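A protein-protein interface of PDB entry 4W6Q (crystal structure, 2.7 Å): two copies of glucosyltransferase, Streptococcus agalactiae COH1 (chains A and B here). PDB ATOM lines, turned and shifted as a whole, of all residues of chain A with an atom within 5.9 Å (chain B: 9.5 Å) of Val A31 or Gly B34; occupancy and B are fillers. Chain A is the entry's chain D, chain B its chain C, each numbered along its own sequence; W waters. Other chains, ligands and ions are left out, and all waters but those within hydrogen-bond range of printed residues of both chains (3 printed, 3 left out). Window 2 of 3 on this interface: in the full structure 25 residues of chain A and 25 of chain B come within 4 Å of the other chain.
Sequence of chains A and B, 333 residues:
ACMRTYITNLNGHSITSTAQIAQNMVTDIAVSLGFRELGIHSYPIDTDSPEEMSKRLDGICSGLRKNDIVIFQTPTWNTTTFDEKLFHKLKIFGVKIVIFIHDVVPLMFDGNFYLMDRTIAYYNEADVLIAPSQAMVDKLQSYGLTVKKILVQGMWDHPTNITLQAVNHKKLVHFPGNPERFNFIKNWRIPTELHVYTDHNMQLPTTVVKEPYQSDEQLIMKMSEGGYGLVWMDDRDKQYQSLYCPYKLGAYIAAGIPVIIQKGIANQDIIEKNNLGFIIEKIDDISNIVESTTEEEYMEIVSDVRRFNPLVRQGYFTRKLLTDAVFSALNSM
Val A31 touches Gly B34 (CG1 to O, 3.9 Å).
NE of Arg B36 touches CG2 of Val A31, at 3.4 Å.
CG2 of Thr B27 touches NH1 of Arg A36, at 3.8 Å.
Arg A36 touches Val B31 (CZ to CG2, 3.7 Å).
Val A31 touches Gly B34, but with the chains exchanged Gly A34 does not touch Val B31 (4.04 Å).
Val A31 touches Arg B36, and with the chains exchanged Arg A36 touches Val B31.
Arg A36 touches Thr B27, but with the chains exchanged Thr A27 does not touch Arg B36 (4.1 Å).
Arg A36 touches Glu B37, and with the chains exchanged Glu A37 touches Arg B36.
Positions printed for both chains: 26, 27, 28, 29, 30, 31, 32, 33, 34, 35, 36 and 37.
Of the 9 pairs that touch across the chains among the printed residues, 6 have their exchanged pair printed and touching as well.
Of the 12 printed residues of chain A, 4 touch a printed residue of chain B.
Hydrophobic or aromatic side chains of chain A that line the printed part of chain B: Val A31.
Along chain A the printed residues that touch a printed residue of chain B span positions 28 to 37.
Of the 21 printed residues of chain B, 7 touch a printed residue of chain A.
Among the printed residues, 9 pairs touch across the chains.
The backbone carbonyl oxygen of Ile B69 lies within hydrogen-bond range of the backbone NH of Tyr B6, at 2.5 Å.
NH1 of Arg B4 is in hydrogen-bond range of OH of Tyr B6, 2.8 Å away.
The backbone carbonyl oxygen (O) of Thr B5 is in hydrogen-bond range of the backbone NH (N) of Arg B36.
N of Ile B7 is in hydrogen-bond range of O of Arg B36 (2.8 Å).
The guanidinium group (NE) of Arg B36 lies within salt-bridge range of the side-chain carboxylate (OE1) of Glu A37, at 3.99 Å.
The guanidinium group of Arg B36 is in salt-bridge range of the side-chain carboxylate of Asp A28 (2.8 Å).
The side-chain carboxylate (OE2) of Glu A37 lies within hydrogen-bond range of the side-chain hydroxyl (OH) of Tyr B6.
The side-chain carboxylate of Glu B37 lies within salt-bridge range of the guanidinium group of Arg A36.
The guanidinium group (NH2) of Arg A36 is in salt-bridge range of the side-chain carboxylate (OD1) of Asp B28, 2.8 Å away.
Water W1 lies within hydrogen-bond range of the backbone carbonyl oxygen of Glu B37 (2.6 Å) and the backbone carbonyl oxygen of Glu A37 (2.6 Å).
Water W2 lies within hydrogen-bond range of the backbone carbonyl oxygen of Phe A35 (2.9 Å) and the backbone carbonyl oxygen of Phe B35 (3.4 Å).
Water W3 lies within hydrogen-bond range of the guanidinium group (NH2) of Arg A36 (3.0 Å) and the side-chain carboxylate (OD1) of Asp B28 (3.3 Å).
Val A31 touches two residues of chain B.
Of the printed residues of chain A, Gly B34 touches Val A31 (3.9 Å).
Of the printed residues of chain A, Glu B37 touches Arg A36.
Printed residues of chain B within 4 Å of Arg A36: Thr B27, Asp B28, Val B31 and Glu B37.
Of the printed residues of chain A, Asp B28 touches Arg A36.
Printed residues of chain A within 4 Å of Arg B36: Asp A28, Val A31 and Glu A37.
Phe A35 touches none of the printed residues of chain B.
The nearest printed residue of chain A that does not touch Glu B37 is Glu A37 (4.2 Å).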
ATOM      1  N   VAL A  26      40.645 -13.716 -32.665  1.00  0.00           N
ATOM      2  CA  VAL A  26      40.296 -15.123 -32.667  1.00  0.00           C
ATOM      3  C   VAL A  26      38.928 -15.363 -32.048  1.00  0.00           C
ATOM      4  O   VAL A  26      38.102 -16.117 -32.574  1.00  0.00           O
ATOM      5  CB  VAL A  26      41.327 -15.935 -31.902  1.00  0.00           C
ATOM      6  CG1 VAL A  26      40.792 -17.331 -31.622  1.00  0.00           C
ATOM      7  CG2 VAL A  26      42.647 -15.963 -32.688  1.00  0.00           C
ATOM      8  N   THR A  27      38.686 -14.686 -30.940  1.00  0.00           N
ATOM      9  CA  THR A  27      37.459 -14.884 -30.192  1.00  0.00           C
ATOM     10  C   THR A  27      36.262 -14.391 -30.981  1.00  0.00           C
ATOM     11  O   THR A  27      35.185 -14.996 -30.946  1.00  0.00           O
ATOM     12  CB  THR A  27      37.533 -14.169 -28.838  1.00  0.00           C
ATOM     13  OG1 THR A  27      38.735 -14.573 -28.176  1.00  0.00           O
ATOM     14  CG2 THR A  27      36.331 -14.514 -27.973  1.00  0.00           C
ATOM     15  N   ASP A  28      36.464 -13.291 -31.697  1.00  0.00           N
ATOM     16  CA  ASP A  28      35.383 -12.678 -32.458  1.00  0.00           C
ATOM     17  C   ASP A  28      35.037 -13.566 -33.644  1.00  0.00           C
ATOM     18  O   ASP A  28      33.868 -13.702 -34.011  1.00  0.00           O
ATOM     19  CB  ASP A  28      35.758 -11.265 -32.900  1.00  0.00           C
ATOM     20  CG  ASP A  28      35.995 -10.331 -31.716  1.00  0.00           C
ATOM     21  OD1 ASP A  28      35.663 -10.703 -30.569  1.00  0.00           O
ATOM     22  OD2 ASP A  28      36.510  -9.218 -31.931  1.00  0.00           O
ATOM     23  N   ILE A  29      36.047 -14.230 -34.193  1.00  0.00           N
ATOM     24  CA  ILE A  29      35.787 -15.269 -35.176  1.00  0.00           C
ATOM     25  C   ILE A  29      35.000 -16.420 -34.531  1.00  0.00           C
ATOM     26  O   ILE A  29      33.968 -16.849 -35.042  1.00  0.00           O
ATOM     27  CB  ILE A  29      37.094 -15.797 -35.800  1.00  0.00           C
ATOM     28  CG1 ILE A  29      37.948 -14.630 -36.262  1.00  0.00           C
ATOM     29  CG2 ILE A  29      36.798 -16.685 -37.002  1.00  0.00           C
ATOM     30  CD1 ILE A  29      37.243 -13.750 -37.295  1.00  0.00           C
ATOM     31  N   ALA A  30      35.490 -16.904 -33.397  1.00  0.00           N
ATOM     32  CA  ALA A  30      34.847 -18.015 -32.698  1.00  0.00           C
ATOM     33  C   ALA A  30      33.358 -17.759 -32.425  1.00  0.00           C
ATOM     34  O   ALA A  30      32.506 -18.601 -32.697  1.00  0.00           O
ATOM     35  CB  ALA A  30      35.572 -18.288 -31.423  1.00  0.00           C
ATOM     36  N   VAL A  31      33.048 -16.587 -31.896  1.00  0.00           N
ATOM     37  CA  VAL A  31      31.666 -16.192 -31.741  1.00  0.00           C
ATOM     38  C   VAL A  31      30.850 -16.324 -33.037  1.00  0.00           C
ATOM     39  O   VAL A  31      29.766 -16.907 -33.033  1.00  0.00           O
ATOM     40  CB  VAL A  31      31.578 -14.770 -31.248  1.00  0.00           C
ATOM     41  CG1 VAL A  31      30.178 -14.243 -31.405  1.00  0.00           C
ATOM     42  CG2 VAL A  31      32.010 -14.708 -29.813  1.00  0.00           C
ATOM     43  N   SER A  32      31.358 -15.799 -34.146  1.00  0.00           N
ATOM     44  CA  SER A  32      30.583 -15.878 -35.379  1.00  0.00           C
ATOM     45  C   SER A  32      30.405 -17.341 -35.804  1.00  0.00           C
ATOM     46  O   SER A  32      29.404 -17.689 -36.439  1.00  0.00           O
ATOM     47  CB  SER A  32      31.228 -15.039 -36.501  1.00  0.00           C
ATOM     48  OG  SER A  32      32.471 -15.563 -36.930  1.00  0.00           O
ATOM     49  N   LEU A  33      31.350 -18.203 -35.431  1.00  0.00           N
ATOM     50  CA  LEU A  33      31.186 -19.636 -35.680  1.00  0.00           C
ATOM     51  C   LEU A  33      30.267 -20.300 -34.661  1.00  0.00           C
ATOM     52  O   LEU A  33      30.013 -21.496 -34.742  1.00  0.00           O
ATOM     53  CB  LEU A  33      32.524 -20.375 -35.657  1.00  0.00           C
ATOM     54  CG  LEU A  33      33.595 -20.173 -36.722  1.00  0.00           C
ATOM     55  CD1 LEU A  33      34.563 -21.342 -36.700  1.00  0.00           C
ATOM     56  CD2 LEU A  33      32.986 -19.998 -38.094  1.00  0.00           C
ATOM     57  N   GLY A  34      29.805 -19.537 -33.678  1.00  0.00           N
ATOM     58  CA  GLY A  34      28.954 -20.084 -32.637  1.00  0.00           C
ATOM     59  C   GLY A  34      29.626 -20.463 -31.319  1.00  0.00           C
ATOM     60  O   GLY A  34      28.942 -20.791 -30.353  1.00  0.00           O
ATOM     61  N   PHE A  35      30.952 -20.433 -31.258  1.00  0.00           N
ATOM     62  CA  PHE A  35      31.647 -20.822 -30.035  1.00  0.00           C
ATOM     63  C   PHE A  35      31.366 -19.783 -28.926  1.00  0.00           C
ATOM     64  O   PHE A  35      30.918 -18.667 -29.209  1.00  0.00           O
ATOM     65  CB  PHE A  35      33.161 -20.962 -30.264  1.00  0.00           C
ATOM     66  CG  PHE A  35      33.560 -21.982 -31.325  1.00  0.00           C
ATOM     67  CD1 PHE A  35      32.626 -22.742 -31.998  1.00  0.00           C
ATOM     68  CD2 PHE A  35      34.907 -22.188 -31.625  1.00  0.00           C
ATOM     69  CE1 PHE A  35      33.020 -23.678 -32.972  1.00  0.00           C
ATOM     70  CE2 PHE A  35      35.300 -23.125 -32.601  1.00  0.00           C
ATOM     71  CZ  PHE A  35      34.355 -23.874 -33.274  1.00  0.00           C
ATOM     72  N   ARG A  36      31.602 -20.162 -27.669  1.00  0.00           N
ATOM     73  CA  ARG A  36      31.353 -19.275 -26.520  1.00  0.00           C
ATOM     74  C   ARG A  36      32.615 -18.884 -25.747  1.00  0.00           C
ATOM     75  O   ARG A  36      33.536 -19.688 -25.591  1.00  0.00           O
ATOM     76  CB  ARG A  36      30.371 -19.924 -25.556  1.00  0.00           C
ATOM     77  CG  ARG A  36      29.086 -20.328 -26.211  1.00  0.00           C
ATOM     78  CD  ARG A  36      28.092 -20.908 -25.208  1.00  0.00           C
ATOM     79  NE  ARG A  36      26.875 -21.333 -25.891  1.00  0.00           N
ATOM     80  CZ  ARG A  36      25.690 -21.478 -25.312  1.00  0.00           C
ATOM     81  NH1 ARG A  36      25.537 -21.212 -24.024  1.00  0.00           N
ATOM     82  NH2 ARG A  36      24.650 -21.868 -26.038  1.00  0.00           N
ATOM     83  N   GLU A  37      32.632 -17.651 -25.251  1.00  0.00           N
ATOM     84  CA  GLU A  37      33.798 -17.095 -24.556  1.00  0.00           C
ATOM     85  C   GLU A  37      33.939 -17.507 -23.086  1.00  0.00           C
ATOM     86  O   GLU A  37      32.989 -17.407 -22.309  1.00  0.00           O
ATOM     87  CB  GLU A  37      33.743 -15.574 -24.632  1.00  0.00           C
ATOM     88  CG  GLU A  37      34.792 -14.851 -23.858  1.00  0.00           C
ATOM     89  CD  GLU A  37      34.558 -13.344 -23.852  1.00  0.00           C
ATOM     90  OE1 GLU A  37      35.147 -12.638 -24.703  1.00  0.00           O
ATOM     91  OE2 GLU A  37      33.773 -12.861 -23.003  1.00  0.00           O
ATOM     92  N   MET B   3      30.873  -2.057 -28.494  1.00  0.00           N
ATOM     93  CA  MET B   3      29.831  -2.695 -27.706  1.00  0.00           C
ATOM     94  C   MET B   3      29.626  -4.171 -28.020  1.00  0.00           C
ATOM     95  O   MET B   3      29.349  -4.540 -29.165  1.00  0.00           O
ATOM     96  CB  MET B   3      28.513  -1.974 -27.916  1.00  0.00           C
ATOM     97  CG  MET B   3      27.494  -2.334 -26.887  1.00  0.00           C
ATOM     98  SD  MET B   3      25.853  -2.361 -27.581  1.00  0.00           S
ATOM     99  CE  MET B   3      25.941  -3.905 -28.492  1.00  0.00           C
ATOM    100  N   ARG B   4      29.761  -5.007 -26.994  1.00  0.00           N
ATOM    101  CA  ARG B   4      29.400  -6.421 -27.085  1.00  0.00           C
ATOM    102  C   ARG B   4      28.219  -6.633 -26.120  1.00  0.00           C
ATOM    103  O   ARG B   4      28.074  -5.885 -25.160  1.00  0.00           O
ATOM    104  CB  ARG B   4      30.622  -7.315 -26.780  1.00  0.00           C
ATOM    105  CG  ARG B   4      31.926  -6.776 -27.429  1.00  0.00           C
ATOM    106  CD  ARG B   4      33.234  -7.244 -26.783  1.00  0.00           C
ATOM    107  NE  ARG B   4      33.371  -6.646 -25.461  1.00  0.00           N
ATOM    108  CZ  ARG B   4      33.908  -7.277 -24.427  1.00  0.00           C
ATOM    109  NH1 ARG B   4      34.390  -8.502 -24.580  1.00  0.00           N
ATOM    110  NH2 ARG B   4      33.950  -6.698 -23.240  1.00  0.00           N
ATOM    111  N   THR B   5      27.334  -7.586 -26.408  1.00  0.00           N
ATOM    112  CA  THR B   5      26.183  -7.843 -25.534  1.00  0.00           C
ATOM    113  C   THR B   5      26.366  -9.147 -24.796  1.00  0.00           C
ATOM    114  O   THR B   5      26.717 -10.157 -25.396  1.00  0.00           O
ATOM    115  CB  THR B   5      24.857  -7.892 -26.300  1.00  0.00           C
ATOM    116  OG1 THR B   5      24.589  -6.597 -26.845  1.00  0.00           O
ATOM    117  CG2 THR B   5      23.733  -8.231 -25.382  1.00  0.00           C
ATOM    118  N   TYR B   6      26.143  -9.111 -23.487  1.00  0.00           N
ATOM    119  CA  TYR B   6      26.262 -10.302 -22.653  1.00  0.00           C
ATOM    120  C   TYR B   6      24.936 -10.710 -22.015  1.00  0.00           C
ATOM    121  O   TYR B   6      24.095  -9.865 -21.695  1.00  0.00           O
ATOM    122  CB  TYR B   6      27.306 -10.085 -21.558  1.00  0.00           C
ATOM    123  CG  TYR B   6      28.733 -10.161 -22.037  1.00  0.00           C
ATOM    124  CD1 TYR B   6      29.367  -9.051 -22.573  1.00  0.00           C
ATOM    125  CD2 TYR B   6      29.449 -11.343 -21.939  1.00  0.00           C
ATOM    126  CE1 TYR B   6      30.687  -9.115 -23.010  1.00  0.00           C
ATOM    127  CE2 TYR B   6      30.759 -11.424 -22.358  1.00  0.00           C
ATOM    128  CZ  TYR B   6      31.378 -10.305 -22.902  1.00  0.00           C
ATOM    129  OH  TYR B   6      32.685 -10.377 -23.334  1.00  0.00           O
ATOM    130  N   ILE B   7      24.757 -12.016 -21.837  1.00  0.00           N
ATOM    131  CA  ILE B   7      23.600 -12.528 -21.106  1.00  0.00           C
ATOM    132  C   ILE B   7      24.030 -13.562 -20.063  1.00  0.00           C
ATOM    133  O   ILE B   7      24.913 -14.397 -20.314  1.00  0.00           O
ATOM    134  CB  ILE B   7      22.555 -13.141 -22.053  1.00  0.00           C
ATOM    135  CG1 ILE B   7      21.224 -13.321 -21.340  1.00  0.00           C
ATOM    136  CG2 ILE B   7      23.026 -14.461 -22.614  1.00  0.00           C
ATOM    137  CD1 ILE B   7      20.170 -13.978 -22.191  1.00  0.00           C
ATOM    138  N   VAL B  26      16.836 -19.498 -23.736  1.00  0.00           N
ATOM    139  CA  VAL B  26      16.932 -18.097 -24.123  1.00  0.00           C
ATOM    140  C   VAL B  26      18.361 -17.779 -24.524  1.00  0.00           C
ATOM    141  O   VAL B  26      18.616 -17.146 -25.556  1.00  0.00           O
ATOM    142  CB  VAL B  26      16.499 -17.159 -22.995  1.00  0.00           C
ATOM    143  CG1 VAL B  26      17.045 -15.742 -23.224  1.00  0.00           C
ATOM    144  CG2 VAL B  26      14.974 -17.167 -22.859  1.00  0.00           C
ATOM    145  N   THR B  27      19.287 -18.248 -23.703  1.00  0.00           N
ATOM    146  CA  THR B  27      20.692 -17.979 -23.913  1.00  0.00           C
ATOM    147  C   THR B  27      21.063 -18.477 -25.289  1.00  0.00           C
ATOM    148  O   THR B  27      21.749 -17.795 -26.057  1.00  0.00           O
ATOM    149  CB  THR B  27      21.543 -18.645 -22.814  1.00  0.00           C
ATOM    150  OG1 THR B  27      21.251 -18.012 -21.564  1.00  0.00           O
ATOM    151  CG2 THR B  27      23.019 -18.518 -23.090  1.00  0.00           C
ATOM    152  N   ASP B  28      20.545 -19.649 -25.611  1.00  0.00           N
ATOM    153  CA  ASP B  28      20.782 -20.263 -26.910  1.00  0.00           C
ATOM    154  C   ASP B  28      20.336 -19.382 -28.074  1.00  0.00           C
ATOM    155  O   ASP B  28      21.050 -19.258 -29.068  1.00  0.00           O
ATOM    156  CB  ASP B  28      20.090 -21.612 -26.970  1.00  0.00           C
ATOM    157  CG  ASP B  28      20.940 -22.711 -26.383  1.00  0.00           C
ATOM    158  OD1 ASP B  28      22.128 -22.794 -26.748  1.00  0.00           O
ATOM    159  OD2 ASP B  28      20.439 -23.485 -25.549  1.00  0.00           O
ATOM    160  N   ILE B  29      19.183 -18.747 -27.953  1.00  0.00           N
ATOM    161  CA  ILE B  29      18.814 -17.753 -28.948  1.00  0.00           C
ATOM    162  C   ILE B  29      19.840 -16.615 -28.969  1.00  0.00           C
ATOM    163  O   ILE B  29      20.369 -16.280 -30.040  1.00  0.00           O
ATOM    164  CB  ILE B  29      17.414 -17.166 -28.711  1.00  0.00           C
ATOM    165  CG1 ILE B  29      16.359 -18.098 -29.254  1.00  0.00           C
ATOM    166  CG2 ILE B  29      17.226 -15.878 -29.474  1.00  0.00           C
ATOM    167  CD1 ILE B  29      16.279 -19.417 -28.556  1.00  0.00           C
ATOM    168  N   ALA B  30      20.131 -16.039 -27.799  1.00  0.00           N
ATOM    169  CA  ALA B  30      21.074 -14.911 -27.693  1.00  0.00           C
ATOM    170  C   ALA B  30      22.417 -15.211 -28.366  1.00  0.00           C
ATOM    171  O   ALA B  30      22.933 -14.395 -29.127  1.00  0.00           O
ATOM    172  CB  ALA B  30      21.285 -14.529 -26.246  1.00  0.00           C
ATOM    173  N   VAL B  31      22.968 -16.390 -28.107  1.00  0.00           N
ATOM    174  CA  VAL B  31      24.184 -16.794 -28.787  1.00  0.00           C
ATOM    175  C   VAL B  31      24.047 -16.660 -30.300  1.00  0.00           C
ATOM    176  O   VAL B  31      24.876 -16.016 -30.947  1.00  0.00           O
ATOM    177  CB  VAL B  31      24.564 -18.229 -28.426  1.00  0.00           C
ATOM    178  CG1 VAL B  31      25.571 -18.781 -29.393  1.00  0.00           C
ATOM    179  CG2 VAL B  31      25.116 -18.285 -27.018  1.00  0.00           C
ATOM    180  N   SER B  32      22.986 -17.226 -30.863  1.00  0.00           N
ATOM    181  CA  SER B  32      22.822 -17.203 -32.317  1.00  0.00           C
ATOM    182  C   SER B  32      22.637 -15.772 -32.821  1.00  0.00           C
ATOM    183  O   SER B  32      22.888 -15.485 -33.988  1.00  0.00           O
ATOM    184  CB  SER B  32      21.644 -18.100 -32.763  1.00  0.00           C
ATOM    185  OG  SER B  32      20.390 -17.436 -32.681  1.00  0.00           O
ATOM    186  N   LEU B  33      22.204 -14.877 -31.943  1.00  0.00           N
ATOM    187  CA  LEU B  33      22.162 -13.462 -32.282  1.00  0.00           C
ATOM    188  C   LEU B  33      23.528 -12.795 -32.114  1.00  0.00           C
ATOM    189  O   LEU B  33      23.636 -11.578 -32.222  1.00  0.00           O
ATOM    190  CB  LEU B  33      21.157 -12.725 -31.410  1.00  0.00           C
ATOM    191  CG  LEU B  33      19.698 -13.136 -31.439  1.00  0.00           C
ATOM    192  CD1 LEU B  33      18.949 -12.330 -30.383  1.00  0.00           C
ATOM    193  CD2 LEU B  33      19.093 -12.944 -32.838  1.00  0.00           C
ATOM    194  N   GLY B  34      24.556 -13.587 -31.829  1.00  0.00           N
ATOM    195  CA  GLY B  34      25.877 -13.054 -31.586  1.00  0.00           C
ATOM    196  C   GLY B  34      26.149 -12.572 -30.163  1.00  0.00           C
ATOM    197  O   GLY B  34      27.248 -12.093 -29.894  1.00  0.00           O
ATOM    198  N   PHE B  35      25.173 -12.689 -29.256  1.00  0.00           N
ATOM    199  CA  PHE B  35      25.377 -12.272 -27.859  1.00  0.00           C
ATOM    200  C   PHE B  35      26.325 -13.284 -27.160  1.00  0.00           C
ATOM    201  O   PHE B  35      26.621 -14.343 -27.718  1.00  0.00           O
ATOM    202  CB  PHE B  35      24.038 -12.123 -27.090  1.00  0.00           C
ATOM    203  CG  PHE B  35      23.078 -11.061 -27.656  1.00  0.00           C
ATOM    204  CD1 PHE B  35      23.359 -10.362 -28.826  1.00  0.00           C
ATOM    205  CD2 PHE B  35      21.873 -10.777 -27.005  1.00  0.00           C
ATOM    206  CE1 PHE B  35      22.453  -9.397 -29.328  1.00  0.00           C
ATOM    207  CE2 PHE B  35      20.961  -9.803 -27.509  1.00  0.00           C
ATOM    208  CZ  PHE B  35      21.254  -9.113 -28.669  1.00  0.00           C
ATOM    209  N   ARG B  36      26.840 -12.943 -25.974  1.00  0.00           N
ATOM    210  CA  ARG B  36      27.807 -13.813 -25.282  1.00  0.00           C
ATOM    211  C   ARG B  36      27.348 -14.299 -23.897  1.00  0.00           C
ATOM    212  O   ARG B  36      26.776 -13.540 -23.117  1.00  0.00           O
ATOM    213  CB  ARG B  36      29.146 -13.097 -25.134  1.00  0.00           C
ATOM    214  CG  ARG B  36      30.032 -13.174 -26.351  1.00  0.00           C
ATOM    215  CD  ARG B  36      31.220 -12.213 -26.245  1.00  0.00           C
ATOM    216  NE  ARG B  36      32.170 -12.397 -27.344  1.00  0.00           N
ATOM    217  CZ  ARG B  36      32.740 -11.410 -28.027  1.00  0.00           C
ATOM    218  NH1 ARG B  36      32.465 -10.149 -27.736  1.00  0.00           N
ATOM    219  NH2 ARG B  36      33.583 -11.687 -29.007  1.00  0.00           N
ATOM    220  N   GLU B  37      27.604 -15.569 -23.601  1.00  0.00           N
ATOM    221  CA  GLU B  37      27.216 -16.144 -22.315  1.00  0.00           C
ATOM    222  C   GLU B  37      28.054 -15.643 -21.140  1.00  0.00           C
ATOM    223  O   GLU B  37      29.280 -15.674 -21.200  1.00  0.00           O
ATOM    224  CB  GLU B  37      27.323 -17.670 -22.367  1.00  0.00           C
ATOM    225  CG  GLU B  37      26.872 -18.380 -21.092  1.00  0.00           C
ATOM    226  CD  GLU B  37      27.375 -19.820 -20.997  1.00  0.00           C
ATOM    227  OE1 GLU B  37      26.559 -20.753 -21.124  1.00  0.00           O
ATOM    228  OE2 GLU B  37      28.583 -20.023 -20.773  1.00  0.00           O
ATOM    229  N   ILE B  69      26.786  -4.244 -23.056  1.00  0.00           N
ATOM    230  CA  ILE B  69      25.455  -4.433 -22.480  1.00  0.00           C
ATOM    231  C   ILE B  69      25.320  -5.818 -21.879  1.00  0.00           C
ATOM    232  O   ILE B  69      25.679  -6.818 -22.509  1.00  0.00           O
ATOM    233  CB  ILE B  69      24.342  -4.250 -23.514  1.00  0.00           C
ATOM    234  CG1 ILE B  69      24.580  -2.968 -24.287  1.00  0.00           C
ATOM    235  CG2 ILE B  69      22.959  -4.224 -22.839  1.00  0.00           C
ATOM    236  CD1 ILE B  69      24.457  -1.745 -23.440  1.00  0.00           C
ATOM    237  N   ARG B 319      13.738 -13.674 -29.509  1.00  0.00           N
ATOM    238  CA  ARG B 319      14.466 -12.823 -30.453  1.00  0.00           C
ATOM    239  C   ARG B 319      13.948 -11.390 -30.366  1.00  0.00           C
ATOM    240  O   ARG B 319      14.720 -10.446 -30.367  1.00  0.00           O
ATOM    241  CB  ARG B 319      14.326 -13.361 -31.886  1.00  0.00           C
ATOM    242  CG  ARG B 319      15.292 -14.486 -32.278  1.00  0.00           C
ATOM    243  CD  ARG B 319      14.890 -15.137 -33.614  1.00  0.00           C
ATOM    244  NE  ARG B 319      16.023 -15.677 -34.375  1.00  0.00           N
ATOM    245  CZ  ARG B 319      16.675 -15.024 -35.352  1.00  0.00           C
ATOM    246  NH1 ARG B 319      16.334 -13.791 -35.717  1.00  0.00           N
ATOM    247  NH2 ARG B 319      17.685 -15.609 -35.978  1.00  0.00           N
ATOM    248  N   LEU B 322      15.017  -9.782 -26.821  1.00  0.00           N
ATOM    249  CA  LEU B 322      16.468  -9.693 -26.835  1.00  0.00           C
ATOM    250  C   LEU B 322      16.992  -8.562 -27.711  1.00  0.00           C
ATOM    251  O   LEU B 322      18.090  -8.038 -27.493  1.00  0.00           O
ATOM    252  CB  LEU B 322      17.077 -10.996 -27.320  1.00  0.00           C
ATOM    253  CG  LEU B 322      17.031 -12.200 -26.390  1.00  0.00           C
ATOM    254  CD1 LEU B 322      17.991 -13.266 -26.906  1.00  0.00           C
ATOM    255  CD2 LEU B 322      17.356 -11.801 -24.969  1.00  0.00           C
ATOM    256  N   THR B 323      16.212  -8.194 -28.712  1.00  0.00           N
ATOM    257  CA  THR B 323      16.628  -7.135 -29.601  1.00  0.00           C
ATOM    258  C   THR B 323      16.137  -5.798 -29.090  1.00  0.00           C
ATOM    259  O   THR B 323      16.921  -4.854 -28.967  1.00  0.00           O
ATOM    260  CB  THR B 323      16.119  -7.380 -31.028  1.00  0.00           C
ATOM    261  OG1 THR B 323      16.601  -8.649 -31.459  1.00  0.00           O
ATOM    262  CG2 THR B 323      16.619  -6.311 -31.987  1.00  0.00           C
HETATM  263  O   HOH W   1      30.649 -16.641 -23.221  1.00  0.00           O
HETATM  264  O   HOH W   2      29.085 -16.595 -28.341  1.00  0.00           O
HETATM  265  O   HOH W   3      24.632 -22.866 -28.918  1.00  0.00           O
